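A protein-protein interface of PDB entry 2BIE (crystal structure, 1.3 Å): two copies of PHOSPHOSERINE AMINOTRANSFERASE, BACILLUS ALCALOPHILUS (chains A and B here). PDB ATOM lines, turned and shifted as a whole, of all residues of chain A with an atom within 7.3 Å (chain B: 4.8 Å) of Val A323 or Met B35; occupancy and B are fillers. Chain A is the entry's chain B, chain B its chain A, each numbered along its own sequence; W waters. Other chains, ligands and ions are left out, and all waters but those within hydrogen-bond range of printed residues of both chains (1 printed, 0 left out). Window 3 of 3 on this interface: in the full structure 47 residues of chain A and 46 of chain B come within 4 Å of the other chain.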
ATOM      1  N   GLN A   4      -1.830  16.588 -10.878  1.00  0.00           N
ATOM      2  CA  GLN A   4      -2.209  18.011 -10.945  1.00  0.00           C
ATOM      3  C   GLN A   4      -1.543  18.653 -12.174  1.00  0.00           C
ATOM      4  O   GLN A   4      -0.321  18.595 -12.337  1.00  0.00           O
ATOM      5  CB  GLN A   4      -1.811  18.875  -9.756  1.00  0.00           C
ATOM      6  CG  GLN A   4      -2.791  19.082  -8.617  1.00  0.00           C
ATOM      7  CD  GLN A   4      -2.269  19.790  -7.384  1.00  0.00           C
ATOM      8  OE1 GLN A   4      -1.087  19.808  -7.018  1.00  0.00           O
ATOM      9  NE2 GLN A   4      -3.199  20.427  -6.659  1.00  0.00           N
ATOM     10  N   VAL A   5      -2.351  19.278 -13.019  1.00  0.00           N
ATOM     11  CA  VAL A   5      -1.934  20.065 -14.155  1.00  0.00           C
ATOM     12  C   VAL A   5      -2.587  21.442 -14.107  1.00  0.00           C
ATOM     13  O   VAL A   5      -3.773  21.553 -13.863  1.00  0.00           O
ATOM     14  CB  VAL A   5      -2.302  19.359 -15.470  1.00  0.00           C
ATOM     15  CG1 VAL A   5      -2.012  20.165 -16.697  1.00  0.00           C
ATOM     16  CG2 VAL A   5      -1.526  18.024 -15.435  1.00  0.00           C
ATOM     17  N   PHE A   6      -1.770  22.466 -14.338  1.00  0.00           N
ATOM     18  CA  PHE A   6      -2.210  23.852 -14.334  1.00  0.00           C
ATOM     19  C   PHE A   6      -1.869  24.465 -15.689  1.00  0.00           C
ATOM     20  O   PHE A   6      -0.686  24.579 -16.034  1.00  0.00           O
ATOM     21  CB  PHE A   6      -1.517  24.610 -13.190  1.00  0.00           C
ATOM     22  CG  PHE A   6      -1.811  23.958 -11.848  1.00  0.00           C
ATOM     23  CD1 PHE A   6      -0.789  23.261 -11.237  1.00  0.00           C
ATOM     24  CD2 PHE A   6      -3.054  24.037 -11.258  1.00  0.00           C
ATOM     25  CE1 PHE A   6      -1.050  22.676 -10.024  1.00  0.00           C
ATOM     26  CE2 PHE A   6      -3.297  23.456 -10.047  1.00  0.00           C
ATOM     27  CZ  PHE A   6      -2.277  22.765  -9.417  1.00  0.00           C
ATOM     28  N   ASN A   7      -2.888  24.793 -16.461  1.00  0.00           N
ATOM     29  CA  ASN A   7      -2.693  25.167 -17.859  1.00  0.00           C
ATOM     30  C   ASN A   7      -2.622  26.670 -18.059  1.00  0.00           C
ATOM     31  O   ASN A   7      -3.633  27.331 -18.194  1.00  0.00           O
ATOM     32  CB  ASN A   7      -3.783  24.553 -18.744  1.00  0.00           C
ATOM     33  CG  ASN A   7      -3.586  24.786 -20.229  1.00  0.00           C
ATOM     34  OD1 ASN A   7      -2.602  25.403 -20.607  1.00  0.00           O
ATOM     35  ND2 ASN A   7      -4.547  24.300 -21.022  1.00  0.00           N
ATOM     36  N   PHE A   8      -1.382  27.167 -18.090  1.00  0.00           N
ATOM     37  CA  PHE A   8      -1.040  28.545 -18.364  1.00  0.00           C
ATOM     38  C   PHE A   8      -0.563  28.736 -19.798  1.00  0.00           C
ATOM     39  O   PHE A   8       0.160  29.686 -20.083  1.00  0.00           O
ATOM     40  CB  PHE A   8       0.008  29.053 -17.381  1.00  0.00           C
ATOM     41  CG  PHE A   8      -0.524  29.247 -15.962  1.00  0.00           C
ATOM     42  CD1 PHE A   8      -0.434  28.238 -15.039  1.00  0.00           C
ATOM     43  CD2 PHE A   8      -1.109  30.448 -15.570  1.00  0.00           C
ATOM     44  CE1 PHE A   8      -0.903  28.380 -13.748  1.00  0.00           C
ATOM     45  CE2 PHE A   8      -1.572  30.590 -14.299  1.00  0.00           C
ATOM     46  CZ  PHE A   8      -1.478  29.583 -13.377  1.00  0.00           C
ATOM     47  N   ASN A   9      -1.007  27.896 -20.719  1.00  0.00           N
ATOM     48  CA  ASN A   9      -0.616  28.077 -22.118  1.00  0.00           C
ATOM     49  C   ASN A   9      -1.092  29.422 -22.650  1.00  0.00           C
ATOM     50  O   ASN A   9      -2.140  29.954 -22.309  1.00  0.00           O
ATOM     51  CB  ASN A   9      -1.191  26.949 -23.013  1.00  0.00           C
ATOM     52  CG  ASN A   9      -0.341  25.711 -23.087  1.00  0.00           C
ATOM     53  OD1 ASN A   9       0.870  25.894 -23.162  1.00  0.00           O
ATOM     54  ND2 ASN A   9      -0.887  24.497 -23.099  1.00  0.00           N
ATOM     55  N   ALA A  10      -0.295  29.960 -23.582  1.00  0.00           N
ATOM     56  CA  ALA A  10      -0.443  31.326 -24.106  1.00  0.00           C
ATOM     57  C   ALA A  10      -1.235  31.419 -25.381  1.00  0.00           C
ATOM     58  O   ALA A  10      -1.497  32.524 -25.854  1.00  0.00           O
ATOM     59  CB  ALA A  10       0.918  32.008 -24.343  1.00  0.00           C
ATOM     60  N   SER A  13      -5.017  27.564 -25.625  1.00  0.00           N
ATOM     61  CA  SER A  13      -5.105  27.790 -24.207  1.00  0.00           C
ATOM     62  C   SER A  13      -6.222  26.973 -23.579  1.00  0.00           C
ATOM     63  O   SER A  13      -7.000  26.280 -24.197  1.00  0.00           O
ATOM     64  CB  SER A  13      -5.448  29.284 -24.031  1.00  0.00           C
ATOM     65  OG  SER A  13      -4.708  30.170 -24.850  1.00  0.00           O
ATOM     66  N   ALA A  14      -6.272  27.095 -22.271  1.00  0.00           N
ATOM     67  CA  ALA A  14      -7.315  26.437 -21.472  1.00  0.00           C
ATOM     68  C   ALA A  14      -8.674  26.848 -21.975  1.00  0.00           C
ATOM     69  O   ALA A  14      -8.898  28.012 -22.353  1.00  0.00           O
ATOM     70  CB  ALA A  14      -7.191  26.895 -20.020  1.00  0.00           C
ATOM     71  N   LYS A  17     -14.107  23.950 -18.565  1.00  0.00           N
ATOM     72  CA  LYS A  17     -14.467  22.540 -18.444  1.00  0.00           C
ATOM     73  C   LYS A  17     -15.896  22.291 -18.890  1.00  0.00           C
ATOM     74  O   LYS A  17     -16.157  21.301 -19.598  1.00  0.00           O
ATOM     75  CB  LYS A  17     -14.251  22.013 -17.020  1.00  0.00           C
ATOM     76  CG  LYS A  17     -12.788  21.833 -16.691  1.00  0.00           C
ATOM     77  CD  LYS A  17     -12.599  20.928 -15.490  1.00  0.00           C
ATOM     78  CE  LYS A  17     -11.315  20.101 -15.532  1.00  0.00           C
ATOM     79  NZ  LYS A  17     -11.096  19.416 -16.838  1.00  0.00           N
ATOM     80  N   LEU A  20     -16.086  21.930 -22.744  1.00  0.00           N
ATOM     81  CA  LEU A  20     -15.482  20.718 -23.239  1.00  0.00           C
ATOM     82  C   LEU A  20     -16.300  19.482 -22.862  1.00  0.00           C
ATOM     83  O   LEU A  20     -16.444  18.587 -23.694  1.00  0.00           O
ATOM     84  CB  LEU A  20     -14.051  20.569 -22.718  1.00  0.00           C
ATOM     85  CG  LEU A  20     -13.037  21.366 -23.556  1.00  0.00           C
ATOM     86  CD1 LEU A  20     -11.707  21.527 -22.818  1.00  0.00           C
ATOM     87  CD2 LEU A  20     -12.796  20.737 -24.928  1.00  0.00           C
ATOM     88  N   ALA A 317       8.474  24.434 -11.825  1.00  0.00           N
ATOM     89  CA  ALA A 317       7.075  24.563 -12.181  1.00  0.00           C
ATOM     90  C   ALA A 317       6.652  23.414 -13.094  1.00  0.00           C
ATOM     91  O   ALA A 317       5.571  22.841 -12.907  1.00  0.00           O
ATOM     92  CB  ALA A 317       6.883  25.891 -12.865  1.00  0.00           C
ATOM     93  N   LYS A 318       7.480  23.112 -14.068  1.00  0.00           N
ATOM     94  CA  LYS A 318       7.099  22.044 -14.961  1.00  0.00           C
ATOM     95  C   LYS A 318       6.995  20.723 -14.210  1.00  0.00           C
ATOM     96  O   LYS A 318       6.091  19.925 -14.486  1.00  0.00           O
ATOM     97  CB  LYS A 318       8.130  21.906 -16.089  1.00  0.00           C
ATOM     98  CG  LYS A 318       7.732  20.917 -17.190  1.00  0.00           C
ATOM     99  CD  LYS A 318       8.709  21.060 -18.365  1.00  0.00           C
ATOM    100  CE  LYS A 318       8.487  19.990 -19.439  1.00  0.00           C
ATOM    101  NZ  LYS A 318       9.778  19.742 -20.186  1.00  0.00           N
ATOM    102  N   GLN A 320       6.065  20.307 -11.232  1.00  0.00           N
ATOM    103  CA  GLN A 320       4.874  20.345 -10.388  1.00  0.00           C
ATOM    104  C   GLN A 320       3.578  20.475 -11.181  1.00  0.00           C
ATOM    105  O   GLN A 320       2.503  20.658 -10.613  1.00  0.00           O
ATOM    106  CB  GLN A 320       5.029  21.517  -9.380  1.00  0.00           C
ATOM    107  CG  GLN A 320       6.184  21.348  -8.395  1.00  0.00           C
ATOM    108  CD  GLN A 320       6.158  20.022  -7.677  1.00  0.00           C
ATOM    109  OE1 GLN A 320       7.030  19.131  -7.615  1.00  0.00           O
ATOM    110  NE2 GLN A 320       5.023  19.852  -7.035  1.00  0.00           N
ATOM    111  N   GLY A 321       3.616  20.364 -12.504  1.00  0.00           N
ATOM    112  CA  GLY A 321       2.477  20.252 -13.372  1.00  0.00           C
ATOM    113  C   GLY A 321       1.998  21.511 -14.031  1.00  0.00           C
ATOM    114  O   GLY A 321       0.936  21.541 -14.650  1.00  0.00           O
ATOM    115  N   PHE A 322       2.774  22.596 -13.893  1.00  0.00           N
ATOM    116  CA  PHE A 322       2.447  23.853 -14.569  1.00  0.00           C
ATOM    117  C   PHE A 322       2.903  23.782 -16.002  1.00  0.00           C
ATOM    118  O   PHE A 322       4.021  23.376 -16.244  1.00  0.00           O
ATOM    119  CB  PHE A 322       3.128  25.044 -13.922  1.00  0.00           C
ATOM    120  CG  PHE A 322       2.626  25.251 -12.497  1.00  0.00           C
ATOM    121  CD1 PHE A 322       3.083  24.525 -11.426  1.00  0.00           C
ATOM    122  CD2 PHE A 322       1.633  26.180 -12.299  1.00  0.00           C
ATOM    123  CE1 PHE A 322       2.612  24.664 -10.134  1.00  0.00           C
ATOM    124  CE2 PHE A 322       1.132  26.363 -11.023  1.00  0.00           C
ATOM    125  CZ  PHE A 322       1.612  25.593  -9.958  1.00  0.00           C
ATOM    126  N   VAL A 323       2.000  24.181 -16.886  1.00  0.00           N
ATOM    127  CA  VAL A 323       2.268  24.159 -18.338  1.00  0.00           C
ATOM    128  C   VAL A 323       2.209  25.539 -18.933  1.00  0.00           C
ATOM    129  O   VAL A 323       1.276  26.281 -18.653  1.00  0.00           O
ATOM    130  CB  VAL A 323       1.214  23.277 -19.011  1.00  0.00           C
ATOM    131  CG1 VAL A 323       1.439  23.246 -20.513  1.00  0.00           C
ATOM    132  CG2 VAL A 323       1.230  21.852 -18.386  1.00  0.00           C
ATOM    133  N   GLY A 324       3.183  25.867 -19.761  1.00  0.00           N
ATOM    134  CA  GLY A 324       3.139  27.093 -20.542  1.00  0.00           C
ATOM    135  C   GLY A 324       3.840  28.294 -19.954  1.00  0.00           C
ATOM    136  O   GLY A 324       3.792  29.360 -20.566  1.00  0.00           O
ATOM    137  N   LEU A 325       4.488  28.214 -18.812  1.00  0.00           N
ATOM    138  CA  LEU A 325       5.035  29.398 -18.126  1.00  0.00           C
ATOM    139  C   LEU A 325       6.310  29.968 -18.750  1.00  0.00           C
ATOM    140  O   LEU A 325       6.721  31.094 -18.387  1.00  0.00           O
ATOM    141  CB  LEU A 325       5.297  29.095 -16.655  1.00  0.00           C
ATOM    142  CG  LEU A 325       4.062  28.860 -15.771  1.00  0.00           C
ATOM    143  CD1 LEU A 325       4.526  28.445 -14.383  1.00  0.00           C
ATOM    144  CD2 LEU A 325       3.159  30.094 -15.769  1.00  0.00           C
ATOM    145  N   ASN A 326       6.962  29.271 -19.665  1.00  0.00           N
ATOM    146  CA  ASN A 326       8.187  29.848 -20.256  1.00  0.00           C
ATOM    147  C   ASN A 326       7.830  31.119 -20.999  1.00  0.00           C
ATOM    148  O   ASN A 326       6.876  31.116 -21.786  1.00  0.00           O
ATOM    149  CB  ASN A 326       8.810  28.889 -21.264  1.00  0.00           C
ATOM    150  CG  ASN A 326       9.337  27.620 -20.663  1.00  0.00           C
ATOM    151  OD1 ASN A 326       9.500  27.452 -19.456  1.00  0.00           O
ATOM    152  ND2 ASN A 326       9.623  26.716 -21.587  1.00  0.00           N
ATOM    153  N   ARG A 335       6.019  33.841 -18.263  1.00  0.00           N
ATOM    154  CA  ARG A 335       4.759  34.432 -18.637  1.00  0.00           C
ATOM    155  C   ARG A 335       3.632  33.518 -18.135  1.00  0.00           C
ATOM    156  O   ARG A 335       3.523  32.367 -18.594  1.00  0.00           O
ATOM    157  CB  ARG A 335       4.672  34.593 -20.120  1.00  0.00           C
ATOM    158  CG  ARG A 335       3.364  35.175 -20.584  1.00  0.00           C
ATOM    159  CD  ARG A 335       3.342  35.502 -22.062  1.00  0.00           C
ATOM    160  NE  ARG A 335       3.680  34.404 -22.920  1.00  0.00           N
ATOM    161  CZ  ARG A 335       3.599  34.431 -24.271  1.00  0.00           C
ATOM    162  NH1 ARG A 335       3.141  35.521 -24.896  1.00  0.00           N
ATOM    163  NH2 ARG A 335       3.981  33.323 -24.943  1.00  0.00           N
ATOM    164  N   SER A 337      -0.073  33.106 -18.497  1.00  0.00           N
ATOM    165  CA  SER A 337      -1.259  33.467 -19.284  1.00  0.00           C
ATOM    166  C   SER A 337      -2.511  33.029 -18.506  1.00  0.00           C
ATOM    167  O   SER A 337      -2.617  31.856 -18.187  1.00  0.00           O
ATOM    168  CB  SER A 337      -1.171  32.890 -20.686  1.00  0.00           C
ATOM    169  OG  SER A 337      -0.037  33.403 -21.403  1.00  0.00           O
ATOM    170  N   LEU B  28     -10.967  15.317 -23.192  1.00  0.00           N
ATOM    171  CA  LEU B  28     -10.549  16.096 -22.051  1.00  0.00           C
ATOM    172  C   LEU B  28      -9.129  15.829 -21.571  1.00  0.00           C
ATOM    173  O   LEU B  28      -8.554  16.658 -20.880  1.00  0.00           O
ATOM    174  CB  LEU B  28     -11.488  15.772 -20.863  1.00  0.00           C
ATOM    175  CG  LEU B  28     -12.990  15.813 -21.145  1.00  0.00           C
ATOM    176  CD1 LEU B  28     -13.824  15.538 -19.876  1.00  0.00           C
ATOM    177  CD2 LEU B  28     -13.358  17.154 -21.780  1.00  0.00           C
ATOM    178  N   ASN B  29      -8.572  14.670 -21.925  1.00  0.00           N
ATOM    179  CA  ASN B  29      -7.255  14.259 -21.450  1.00  0.00           C
ATOM    180  C   ASN B  29      -6.551  13.583 -22.624  1.00  0.00           C
ATOM    181  O   ASN B  29      -6.702  12.369 -22.783  1.00  0.00           O
ATOM    182  CB  ASN B  29      -7.384  13.324 -20.267  1.00  0.00           C
ATOM    183  CG  ASN B  29      -6.062  12.740 -19.819  1.00  0.00           C
ATOM    184  OD1 ASN B  29      -5.002  13.255 -20.167  1.00  0.00           O
ATOM    185  ND2 ASN B  29      -6.155  11.648 -19.084  1.00  0.00           N
ATOM    186  N   PHE B  30      -5.829  14.360 -23.387  1.00  0.00           N
ATOM    187  CA  PHE B  30      -5.109  13.869 -24.549  1.00  0.00           C
ATOM    188  C   PHE B  30      -3.696  13.469 -24.170  1.00  0.00           C
ATOM    189  O   PHE B  30      -2.970  14.277 -23.581  1.00  0.00           O
ATOM    190  CB  PHE B  30      -5.055  14.985 -25.612  1.00  0.00           C
ATOM    191  CG  PHE B  30      -4.289  14.495 -26.827  1.00  0.00           C
ATOM    192  CD1 PHE B  30      -4.806  13.454 -27.621  1.00  0.00           C
ATOM    193  CD2 PHE B  30      -3.075  15.040 -27.157  1.00  0.00           C
ATOM    194  CE1 PHE B  30      -4.092  12.978 -28.698  1.00  0.00           C
ATOM    195  CE2 PHE B  30      -2.363  14.569 -28.233  1.00  0.00           C
ATOM    196  CZ  PHE B  30      -2.886  13.549 -28.988  1.00  0.00           C
ATOM    197  N   THR B  33      -1.870  14.192 -20.788  1.00  0.00           N
ATOM    198  CA  THR B  33      -1.548  15.557 -20.408  1.00  0.00           C
ATOM    199  C   THR B  33      -2.589  16.199 -19.476  1.00  0.00           C
ATOM    200  O   THR B  33      -2.245  17.246 -18.912  1.00  0.00           O
ATOM    201  CB  THR B  33      -1.404  16.518 -21.603  1.00  0.00           C
ATOM    202  OG1 THR B  33      -2.674  16.656 -22.263  1.00  0.00           O
ATOM    203  CG2 THR B  33      -0.359  16.013 -22.583  1.00  0.00           C
ATOM    204  N   GLN B  34      -3.776  15.609 -19.376  1.00  0.00           N
ATOM    205  CA  GLN B  34      -4.881  16.195 -18.623  1.00  0.00           C
ATOM    206  C   GLN B  34      -5.422  17.481 -19.272  1.00  0.00           C
ATOM    207  O   GLN B  34      -6.147  18.241 -18.606  1.00  0.00           O
ATOM    208  CB  GLN B  34      -4.484  16.429 -17.160  1.00  0.00           C
ATOM    209  CG  GLN B  34      -4.048  15.135 -16.497  1.00  0.00           C
ATOM    210  CD  GLN B  34      -5.102  14.043 -16.496  1.00  0.00           C
ATOM    211  OE1 GLN B  34      -6.305  14.316 -16.528  1.00  0.00           O
ATOM    212  NE2 GLN B  34      -4.637  12.787 -16.441  1.00  0.00           N
ATOM    213  N   MET B  35      -5.097  17.690 -20.542  1.00  0.00           N
ATOM    214  CA  MET B  35      -5.651  18.768 -21.329  1.00  0.00           C
ATOM    215  C   MET B  35      -6.245  18.188 -22.609  1.00  0.00           C
ATOM    216  O   MET B  35      -5.786  17.137 -23.125  1.00  0.00           O
ATOM    217  CB  MET B  35      -4.580  19.770 -21.728  1.00  0.00           C
ATOM    218  CG  MET B  35      -3.960  20.514 -20.546  1.00  0.00           C
ATOM    219  SD  MET B  35      -2.510  21.511 -20.945  1.00  0.00           S
ATOM    220  CE  MET B  35      -1.307  20.188 -20.965  1.00  0.00           C
ATOM    221  N   SER B  36      -7.219  18.854 -23.182  1.00  0.00           N
ATOM    222  CA  SER B  36      -7.687  18.528 -24.504  1.00  0.00           C
ATOM    223  C   SER B  36      -6.624  18.801 -25.565  1.00  0.00           C
ATOM    224  O   SER B  36      -5.816  19.737 -25.345  1.00  0.00           O
ATOM    225  CB  SER B  36      -8.904  19.379 -24.847  1.00  0.00           C
ATOM    226  OG  SER B  36      -9.416  19.037 -26.136  1.00  0.00           O
ATOM    227  N   VAL B  37      -6.617  18.134 -26.689  1.00  0.00           N
ATOM    228  CA  VAL B  37      -5.746  18.546 -27.776  1.00  0.00           C
ATOM    229  C   VAL B  37      -6.012  20.005 -28.104  1.00  0.00           C
ATOM    230  O   VAL B  37      -5.084  20.682 -28.518  1.00  0.00           O
ATOM    231  CB  VAL B  37      -5.782  17.502 -28.909  1.00  0.00           C
ATOM    232  CG1 VAL B  37      -7.099  17.656 -29.629  1.00  0.00           C
ATOM    233  CG2 VAL B  37      -4.621  17.622 -29.887  1.00  0.00           C
ATOM    234  N   GLU B  39      -6.492  22.455 -26.125  1.00  0.00           N
ATOM    235  CA  GLU B  39      -5.941  23.299 -25.065  1.00  0.00           C
ATOM    236  C   GLU B  39      -4.431  23.303 -25.031  1.00  0.00           C
ATOM    237  O   GLU B  39      -3.861  23.976 -24.124  1.00  0.00           O
ATOM    238  CB  GLU B  39      -6.436  22.790 -23.700  1.00  0.00           C
ATOM    239  CG  GLU B  39      -7.956  22.992 -23.525  1.00  0.00           C
ATOM    240  CD  GLU B  39      -8.408  22.403 -22.204  1.00  0.00           C
ATOM    241  OE1 GLU B  39      -8.283  21.161 -22.007  1.00  0.00           O
ATOM    242  OE2 GLU B  39      -8.844  23.203 -21.334  1.00  0.00           O
ATOM    243  N   LEU B  40      -3.794  22.581 -25.945  1.00  0.00           N
ATOM    244  CA  LEU B  40      -2.344  22.452 -25.989  1.00  0.00           C
ATOM    245  C   LEU B  40      -1.703  23.539 -26.850  1.00  0.00           C
ATOM    246  O   LEU B  40      -2.298  24.017 -27.804  1.00  0.00           O
ATOM    247  CB  LEU B  40      -1.943  21.143 -26.649  1.00  0.00           C
ATOM    248  CG  LEU B  40      -2.333  19.845 -25.968  1.00  0.00           C
ATOM    249  CD1 LEU B  40      -1.926  18.650 -26.829  1.00  0.00           C
ATOM    250  CD2 LEU B  40      -1.729  19.777 -24.565  1.00  0.00           C
HETATM  251  O   HOH W   1      -6.802  23.092 -19.463  1.00  0.00           O
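The side-chain amide nitrogen (ND2) of Asn A7 sits at hydrogen-bond distance from the side-chain sulfur (SD) of Met B35. The side-chain amide nitrogen (ND2) of Asn A7 is in hydrogen-bond range of the backbone carbonyl oxygen (O) of Glu B39 (3.2 Å). The backbone carbonyl oxygen (O) of Glu B39 is in hydrogen-bond range of the side-chain amide nitrogen (ND2) of Asn A9.
O of Leu B28 is in hydrogen-bond range of N of Ser B36 (3.5 Å). The backbone NH (N) of Gln B34 is in hydrogen-bond range of the side-chain amide oxygen (OD1) of Asn B29 (2.8 Å). The side-chain hydroxyl (OG1) of Thr B33 sits at hydrogen-bond distance from the backbone carbonyl oxygen (O) of Phe B30. N of Met B35 sits close to OG1 of Thr B33. The backbone carbonyl oxygen (O) of Phe A6 lies within hydrogen-bond range of the backbone NH (N) of Val A323. OD1 of Asn A7 lies within hydrogen-bond range of N of Asn A9 (3.0 Å).
Among the printed residues, merely in contact across the chains: Val A5 with Thr B33 (3.6 Å), Val A5 with Gln B34 (3.8 Å), Asn A9 with Leu B40 (3.8 Å), Ser A13 with Glu B39 (3.3 Å), Ala A14 with Glu B39 (3.6 Å), Leu A20 with Leu B28 (3.6 Å), Leu A20 with Ser B36 (3.97 Å), Leu A20 with Glu B39 (3.5 Å) and Val A323 with Met B35 (3.98 Å).
Of the printed residues of chain B, Val A323 touches Met B35. Printed residues of chain A within 4 Å of Met B35: Asn A7 (3.5 Å) and Val A323 (3.98 Å). Of the printed residues of chain A, Leu B40 touches Asn A9. Of the printed residues of chain A, Leu B28 touches Leu A20 (3.6 Å). Of the printed residues of chain B, Asn A9 touches Glu B39 and Leu B40. Ala A317 touches none of the printed residues of chain B. The nearest printed residue of chain B that does not touch Val A323 is Thr B33 (5.8 Å). The nearest printed residue of chain A that does not touch Met B35 is Asn A9 (4.02 Å). The nearest printed residue of chain A that does not touch Ser B36 is Asn A7 (6.4 Å).
Printed residues of chain B that touch a printed residue of chain A: Leu B28, Thr B33, Gln B34, Met B35, Ser B36, Glu B39 and Leu B40. Among the printed residues, 12 pairs touch across the chains.
No position is printed for both chains.
Water W1 bridges OE2 of Glu B39 and ND2 of Asn A7.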
